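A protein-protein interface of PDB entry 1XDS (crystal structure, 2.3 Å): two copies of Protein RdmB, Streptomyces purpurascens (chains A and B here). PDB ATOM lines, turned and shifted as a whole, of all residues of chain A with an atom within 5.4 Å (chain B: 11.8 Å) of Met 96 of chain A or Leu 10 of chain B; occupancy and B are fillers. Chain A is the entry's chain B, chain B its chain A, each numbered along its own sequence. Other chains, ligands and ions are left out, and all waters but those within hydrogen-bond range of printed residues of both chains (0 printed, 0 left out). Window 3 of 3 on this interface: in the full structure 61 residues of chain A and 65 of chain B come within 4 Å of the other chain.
The guanidinium group (NH2) of Arg 93 of chain A is in salt-bridge range of the side-chain carboxylate (OD1) of Asp 16 of chain B (3.3 Å).
The side-chain hydroxyl (OG1) of Thr 13 of chain B is in hydrogen-bond range of the backbone NH (N) of Gln 15 of chain B, 3.1 Å away. The side-chain hydroxyl (OG1) of Thr 13 of chain B sits at hydrogen-bond distance from the side-chain carboxylate (OD2) of Asp 16 of chain B (2.7 Å). The backbone NH (N) of Leu 94 of chain A sits at hydrogen-bond distance from the side-chain hydroxyl (OG1) of Thr 92 of chain A (3.2 Å).
Among the printed residues, pairs that only touch across the chains: Arg 93 of chain A with Glu 11 of chain B, Arg 93 of chain A with Pro 12 of chain B, Arg 93 of chain A with Thr 13 of chain B, Leu 94 of chain A with Asp 16 of chain B, Met 96 of chain A with Leu 10 of chain B, Met 96 of chain A with Pro 12 of chain B, Leu 97 of chain A with Pro 12 of chain B, Leu 97 of chain A with Asp 16 of chain B, Leu 97 of chain A with Leu 17 of chain B and His 102 of chain A with Pro 12 of chain B.
No residue of chain B comes within 4 Å of Pro 91 of chain A. No residue of chain B comes within 4 Å of Thr 92 of chain A. Arg 93 of chain A touches four residues of chain B. Met 96 of chain A touches just these residues of chain B: Leu 10 (3.8 Å) and Pro 12 (3.7 Å). Leu 97 of chain A touches just these residues of chain B: Pro 12 (3.6 Å), Asp 16 (3.5 Å) and Leu 17 (3.6 Å). Leu 98 of chain A touches none of the printed residues of chain B. His 102 of chain A touches just one residue of chain B: Pro 12 (3.9 Å). Leu 10 of chain B touches just one residue of chain A: Met 96 (3.8 Å). Of the printed residues of chain A, Glu 11 of chain B touches Arg 93 (3.4 Å). Of the printed residues of chain A, Pro 12 of chain B touches Arg 93, Met 96, Leu 97 and His 102. Of the printed residues of chain A, Thr 13 of chain B touches Arg 93 (3.6 Å). Printed residues of chain A within 4 Å of Asp 16 of chain B: Arg 93, Leu 94 and Leu 97. Printed residues of chain A within 4 Å of Leu 17 of chain B: Leu 97 (3.6 Å). The nearest residue of chain A that does not touch Leu 10 of chain B is Arg 93 of chain A (4.1 Å). The nearest printed residue of chain A that does not touch Pro 12 of chain B is Leu 94 of chain A (5.2 Å).
Hydrophobic or aromatic side chains of chain A within 4 Å of the printed part of chain B: Leu 94, Met 96, Leu 97 and His 102. Of the 12 printed residues of chain B, 6 touch a printed residue of chain A. Among the printed residues, Asp or Glu carboxylates within 4 Å of a Lys or Arg side-chain nitrogen of the other chain: Arg 93 of chain A with Asp 16 of chain B (3.3 Å).
No position is printed for both chains. Of the 11 pairs that touch across the chains among the printed residues, none has its exchanged pair printed and touching as well.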
ATOM      1  N   VAL A  42      32.609  -0.842 -17.874  1.00  0.00           N
ATOM      2  CA  VAL A  42      31.742   0.340 -17.989  1.00  0.00           C
ATOM      3  C   VAL A  42      30.885   0.634 -16.718  1.00  0.00           C
ATOM      4  O   VAL A  42      30.228   1.680 -16.631  1.00  0.00           O
ATOM      5  CB  VAL A  42      30.879   0.225 -19.267  1.00  0.00           C
ATOM      6  CG1 VAL A  42      29.798   1.282 -19.335  1.00  0.00           C
ATOM      7  CG2 VAL A  42      31.786   0.310 -20.509  1.00  0.00           C
ATOM      8  N   LEU A  46      32.667   3.370 -12.921  1.00  0.00           N
ATOM      9  CA  LEU A  46      31.678   4.210 -12.250  1.00  0.00           C
ATOM     10  C   LEU A  46      31.385   3.646 -10.870  1.00  0.00           C
ATOM     11  O   LEU A  46      30.769   4.308 -10.048  1.00  0.00           O
ATOM     12  CB  LEU A  46      30.388   4.293 -13.083  1.00  0.00           C
ATOM     13  CG  LEU A  46      30.550   4.286 -14.614  1.00  0.00           C
ATOM     14  CD1 LEU A  46      29.240   4.655 -15.300  1.00  0.00           C
ATOM     15  CD2 LEU A  46      31.685   5.208 -15.065  1.00  0.00           C
ATOM     16  N   PRO A  91      34.051   5.448 -20.333  1.00  0.00           N
ATOM     17  CA  PRO A  91      33.377   4.908 -21.519  1.00  0.00           C
ATOM     18  C   PRO A  91      32.914   5.978 -22.513  1.00  0.00           C
ATOM     19  O   PRO A  91      32.683   7.129 -22.124  1.00  0.00           O
ATOM     20  CB  PRO A  91      32.163   4.209 -20.914  1.00  0.00           C
ATOM     21  CG  PRO A  91      32.652   3.715 -19.590  1.00  0.00           C
ATOM     22  CD  PRO A  91      33.634   4.746 -19.105  1.00  0.00           C
ATOM     23  N   THR A  92      32.778   5.606 -23.782  1.00  0.00           N
ATOM     24  CA  THR A  92      32.244   6.524 -24.775  1.00  0.00           C
ATOM     25  C   THR A  92      30.749   6.261 -24.844  1.00  0.00           C
ATOM     26  O   THR A  92      30.225   5.462 -24.070  1.00  0.00           O
ATOM     27  CB  THR A  92      32.933   6.366 -26.181  1.00  0.00           C
ATOM     28  OG1 THR A  92      32.305   5.330 -26.953  1.00  0.00           O
ATOM     29  CG2 THR A  92      34.388   5.918 -26.065  1.00  0.00           C
ATOM     30  N   ARG A  93      30.069   6.949 -25.756  1.00  0.00           N
ATOM     31  CA  ARG A  93      28.666   6.684 -26.030  1.00  0.00           C
ATOM     32  C   ARG A  93      28.468   5.204 -26.371  1.00  0.00           C
ATOM     33  O   ARG A  93      27.660   4.526 -25.759  1.00  0.00           O
ATOM     34  CB  ARG A  93      28.188   7.564 -27.182  1.00  0.00           C
ATOM     35  CG  ARG A  93      26.689   7.550 -27.402  1.00  0.00           C
ATOM     36  CD  ARG A  93      26.230   8.588 -28.395  1.00  0.00           C
ATOM     37  NE  ARG A  93      26.407   8.122 -29.770  1.00  0.00           N
ATOM     38  CZ  ARG A  93      27.159   8.709 -30.699  1.00  0.00           C
ATOM     39  NH1 ARG A  93      27.850   9.814 -30.434  1.00  0.00           N
ATOM     40  NH2 ARG A  93      27.228   8.175 -31.914  1.00  0.00           N
ATOM     41  N   LEU A  94      29.233   4.722 -27.344  1.00  0.00           N
ATOM     42  CA  LEU A  94      29.299   3.303 -27.703  1.00  0.00           C
ATOM     43  C   LEU A  94      29.637   2.439 -26.494  1.00  0.00           C
ATOM     44  O   LEU A  94      29.035   1.392 -26.284  1.00  0.00           O
ATOM     45  CB  LEU A  94      30.358   3.119 -28.801  1.00  0.00           C
ATOM     46  CG  LEU A  94      30.607   1.817 -29.578  1.00  0.00           C
ATOM     47  CD1 LEU A  94      30.552   0.567 -28.723  1.00  0.00           C
ATOM     48  CD2 LEU A  94      29.675   1.705 -30.770  1.00  0.00           C
ATOM     49  N   GLY A  95      30.608   2.871 -25.703  1.00  0.00           N
ATOM     50  CA  GLY A  95      31.027   2.133 -24.522  1.00  0.00           C
ATOM     51  C   GLY A  95      29.904   1.849 -23.537  1.00  0.00           C
ATOM     52  O   GLY A  95      29.932   0.846 -22.839  1.00  0.00           O
ATOM     53  N   MET A  96      28.903   2.722 -23.485  1.00  0.00           N
ATOM     54  CA  MET A  96      27.791   2.557 -22.548  1.00  0.00           C
ATOM     55  C   MET A  96      26.995   1.261 -22.785  1.00  0.00           C
ATOM     56  O   MET A  96      26.267   0.827 -21.905  1.00  0.00           O
ATOM     57  CB  MET A  96      26.841   3.756 -22.612  1.00  0.00           C
ATOM     58  CG  MET A  96      26.594   4.401 -21.279  1.00  0.00           C
ATOM     59  SD  MET A  96      27.948   5.407 -20.765  1.00  0.00           S
ATOM     60  CE  MET A  96      28.664   4.380 -19.274  1.00  0.00           C
ATOM     61  N   LEU A  97      27.132   0.649 -23.962  1.00  0.00           N
ATOM     62  CA  LEU A  97      26.395  -0.570 -24.273  1.00  0.00           C
ATOM     63  C   LEU A  97      26.742  -1.737 -23.363  1.00  0.00           C
ATOM     64  O   LEU A  97      25.987  -2.704 -23.291  1.00  0.00           O
ATOM     65  CB  LEU A  97      26.580  -0.964 -25.745  1.00  0.00           C
ATOM     66  CG  LEU A  97      25.763  -0.115 -26.718  1.00  0.00           C
ATOM     67  CD1 LEU A  97      25.911  -0.601 -28.133  1.00  0.00           C
ATOM     68  CD2 LEU A  97      24.299  -0.107 -26.336  1.00  0.00           C
ATOM     69  N   LEU A  98      27.873  -1.646 -22.669  1.00  0.00           N
ATOM     70  CA  LEU A  98      28.235  -2.621 -21.644  1.00  0.00           C
ATOM     71  C   LEU A  98      27.823  -2.150 -20.244  1.00  0.00           C
ATOM     72  O   LEU A  98      28.282  -2.701 -19.241  1.00  0.00           O
ATOM     73  CB  LEU A  98      29.744  -2.903 -21.676  1.00  0.00           C
ATOM     74  CG  LEU A  98      30.438  -3.265 -23.002  1.00  0.00           C
ATOM     75  CD1 LEU A  98      31.645  -4.165 -22.713  1.00  0.00           C
ATOM     76  CD2 LEU A  98      29.522  -3.927 -24.020  1.00  0.00           C
ATOM     77  N   ALA A  99      26.958  -1.133 -20.186  1.00  0.00           N
ATOM     78  CA  ALA A  99      26.380  -0.661 -18.928  1.00  0.00           C
ATOM     79  C   ALA A  99      25.341  -1.682 -18.519  1.00  0.00           C
ATOM     80  O   ALA A  99      24.477  -2.023 -19.312  1.00  0.00           O
ATOM     81  CB  ALA A  99      25.729   0.723 -19.100  1.00  0.00           C
ATOM     82  N   HIS A 102      21.563  -0.939 -19.369  1.00  0.00           N
ATOM     83  CA  HIS A 102      21.102  -0.687 -20.739  1.00  0.00           C
ATOM     84  C   HIS A 102      20.127  -1.777 -21.224  1.00  0.00           C
ATOM     85  O   HIS A 102      20.386  -2.957 -20.997  1.00  0.00           O
ATOM     86  CB  HIS A 102      22.290  -0.592 -21.708  1.00  0.00           C
ATOM     87  CG  HIS A 102      21.943   0.057 -23.008  1.00  0.00           C
ATOM     88  ND1 HIS A 102      21.884  -0.638 -24.193  1.00  0.00           N
ATOM     89  CD2 HIS A 102      21.589   1.331 -23.301  1.00  0.00           C
ATOM     90  CE1 HIS A 102      21.528   0.182 -25.165  1.00  0.00           C
ATOM     91  NE2 HIS A 102      21.340   1.383 -24.650  1.00  0.00           N
ATOM     92  N   LEU B  10      26.212   9.581 -21.848  1.00  0.00           N
ATOM     93  CA  LEU B  10      25.365   9.740 -23.073  1.00  0.00           C
ATOM     94  C   LEU B  10      24.576   8.459 -23.377  1.00  0.00           C
ATOM     95  O   LEU B  10      24.786   7.403 -22.754  1.00  0.00           O
ATOM     96  CB  LEU B  10      26.224  10.116 -24.302  1.00  0.00           C
ATOM     97  CG  LEU B  10      26.879  11.505 -24.456  1.00  0.00           C
ATOM     98  CD1 LEU B  10      26.873  11.943 -25.933  1.00  0.00           C
ATOM     99  CD2 LEU B  10      26.245  12.590 -23.570  1.00  0.00           C
ATOM    100  N   GLU B  11      23.682   8.590 -24.359  1.00  0.00           N
ATOM    101  CA  GLU B  11      22.764   7.544 -24.793  1.00  0.00           C
ATOM    102  C   GLU B  11      23.229   6.922 -26.127  1.00  0.00           C
ATOM    103  O   GLU B  11      23.262   7.613 -27.152  1.00  0.00           O
ATOM    104  CB  GLU B  11      21.363   8.160 -24.963  1.00  0.00           C
ATOM    105  N   PRO B  12      23.597   5.636 -26.112  1.00  0.00           N
ATOM    106  CA  PRO B  12      23.912   4.890 -27.346  1.00  0.00           C
ATOM    107  C   PRO B  12      22.821   4.907 -28.437  1.00  0.00           C
ATOM    108  O   PRO B  12      21.709   4.464 -28.177  1.00  0.00           O
ATOM    109  CB  PRO B  12      24.134   3.451 -26.844  1.00  0.00           C
ATOM    110  CG  PRO B  12      24.433   3.567 -25.388  1.00  0.00           C
ATOM    111  CD  PRO B  12      23.798   4.819 -24.901  1.00  0.00           C
ATOM    112  N   THR B  13      23.143   5.404 -29.636  1.00  0.00           N
ATOM    113  CA  THR B  13      22.212   5.354 -30.781  1.00  0.00           C
ATOM    114  C   THR B  13      22.107   3.952 -31.366  1.00  0.00           C
ATOM    115  O   THR B  13      22.786   3.027 -30.916  1.00  0.00           O
ATOM    116  CB  THR B  13      22.577   6.375 -31.946  1.00  0.00           C
ATOM    117  OG1 THR B  13      23.494   5.786 -32.883  1.00  0.00           O
ATOM    118  CG2 THR B  13      23.285   7.644 -31.439  1.00  0.00           C
ATOM    119  N   ASP B  14      21.248   3.811 -32.374  1.00  0.00           N
ATOM    120  CA  ASP B  14      21.045   2.541 -33.065  1.00  0.00           C
ATOM    121  C   ASP B  14      22.331   2.111 -33.743  1.00  0.00           C
ATOM    122  O   ASP B  14      22.695   0.946 -33.708  1.00  0.00           O
ATOM    123  CB  ASP B  14      19.956   2.682 -34.141  1.00  0.00           C
ATOM    124  CG  ASP B  14      18.547   2.800 -33.559  1.00  0.00           C
ATOM    125  OD1 ASP B  14      18.392   2.789 -32.310  1.00  0.00           O
ATOM    126  OD2 ASP B  14      17.536   2.906 -34.292  1.00  0.00           O
ATOM    127  N   GLN B  15      22.986   3.080 -34.378  1.00  0.00           N
ATOM    128  CA  GLN B  15      24.213   2.884 -35.154  1.00  0.00           C
ATOM    129  C   GLN B  15      25.324   2.215 -34.331  1.00  0.00           C
ATOM    130  O   GLN B  15      26.104   1.412 -34.860  1.00  0.00           O
ATOM    131  CB  GLN B  15      24.704   4.245 -35.694  1.00  0.00           C
ATOM    132  CG  GLN B  15      25.311   4.224 -37.089  1.00  0.00           C
ATOM    133  CD  GLN B  15      26.837   4.296 -37.068  1.00  0.00           C
ATOM    134  OE1 GLN B  15      27.430   5.215 -37.648  1.00  0.00           O
ATOM    135  NE2 GLN B  15      27.471   3.330 -36.398  1.00  0.00           N
ATOM    136  N   ASP B  16      25.372   2.543 -33.041  1.00  0.00           N
ATOM    137  CA  ASP B  16      26.415   2.070 -32.134  1.00  0.00           C
ATOM    138  C   ASP B  16      26.170   0.625 -31.693  1.00  0.00           C
ATOM    139  O   ASP B  16      27.117  -0.106 -31.356  1.00  0.00           O
ATOM    140  CB  ASP B  16      26.488   2.969 -30.896  1.00  0.00           C
ATOM    141  CG  ASP B  16      26.510   4.439 -31.240  1.00  0.00           C
ATOM    142  OD1 ASP B  16      27.579   4.939 -31.633  1.00  0.00           O
ATOM    143  OD2 ASP B  16      25.498   5.170 -31.158  1.00  0.00           O
ATOM    144  N   LEU B  17      24.898   0.232 -31.656  1.00  0.00           N
ATOM    145  CA  LEU B  17      24.524  -1.155 -31.412  1.00  0.00           C
ATOM    146  C   LEU B  17      24.855  -2.012 -32.624  1.00  0.00           C
ATOM    147  O   LEU B  17      25.348  -3.126 -32.477  1.00  0.00           O
ATOM    148  CB  LEU B  17      23.030  -1.268 -31.114  1.00  0.00           C
ATOM    149  CG  LEU B  17      22.524  -2.681 -30.807  1.00  0.00           C
ATOM    150  CD1 LEU B  17      23.117  -3.199 -29.517  1.00  0.00           C
ATOM    151  CD2 LEU B  17      20.995  -2.700 -30.760  1.00  0.00           C
ATOM    152  N   ASP B  18      24.544  -1.485 -33.808  1.00  0.00           N
ATOM    153  CA  ASP B  18      24.850  -2.127 -35.086  1.00  0.00           C
ATOM    154  C   ASP B  18      26.346  -2.483 -35.160  1.00  0.00           C
ATOM    155  O   ASP B  18      26.703  -3.587 -35.554  1.00  0.00           O
ATOM    156  CB  ASP B  18      24.470  -1.191 -36.237  1.00  0.00           C
ATOM    157  CG  ASP B  18      24.363  -1.900 -37.566  1.00  0.00           C
ATOM    158  OD1 ASP B  18      23.615  -2.896 -37.664  1.00  0.00           O
ATOM    159  OD2 ASP B  18      24.972  -1.519 -38.589  1.00  0.00           O
ATOM    160  N   VAL B  19      27.198  -1.548 -34.735  1.00  0.00           N
ATOM    161  CA  VAL B  19      28.640  -1.712 -34.818  1.00  0.00           C
ATOM    162  C   VAL B  19      29.139  -2.787 -33.847  1.00  0.00           C
ATOM    163  O   VAL B  19      29.954  -3.625 -34.215  1.00  0.00           O
ATOM    164  CB  VAL B  19      29.375  -0.364 -34.578  1.00  0.00           C
ATOM    165  CG1 VAL B  19      30.880  -0.572 -34.455  1.00  0.00           C
ATOM    166  CG2 VAL B  19      29.083   0.614 -35.714  1.00  0.00           C
ATOM    167  N   LEU B  20      28.645  -2.763 -32.615  1.00  0.00           N
ATOM    168  CA  LEU B  20      29.050  -3.747 -31.616  1.00  0.00           C
ATOM    169  C   LEU B  20      28.690  -5.170 -32.039  1.00  0.00           C
ATOM    170  O   LEU B  20      29.465  -6.094 -31.825  1.00  0.00           O
ATOM    171  CB  LEU B  20      28.408  -3.427 -30.267  1.00  0.00           C
ATOM    172  CG  LEU B  20      28.719  -4.355 -29.090  1.00  0.00           C
ATOM    173  CD1 LEU B  20      30.056  -4.036 -28.466  1.00  0.00           C
ATOM    174  CD2 LEU B  20      27.619  -4.270 -28.057  1.00  0.00           C
ATOM    175  N   LEU B  24      32.659  -5.214 -33.523  1.00  0.00           N
ATOM    176  CA  LEU B  24      33.491  -5.278 -32.314  1.00  0.00           C
ATOM    177  C   LEU B  24      33.236  -6.482 -31.399  1.00  0.00           C
ATOM    178  O   LEU B  24      34.143  -6.925 -30.694  1.00  0.00           O
ATOM    179  CB  LEU B  24      33.304  -4.001 -31.480  1.00  0.00           C
ATOM    180  CG  LEU B  24      33.611  -2.657 -32.143  1.00  0.00           C
ATOM    181  CD1 LEU B  24      33.354  -1.534 -31.130  1.00  0.00           C
ATOM    182  CD2 LEU B  24      35.030  -2.563 -32.677  1.00  0.00           C
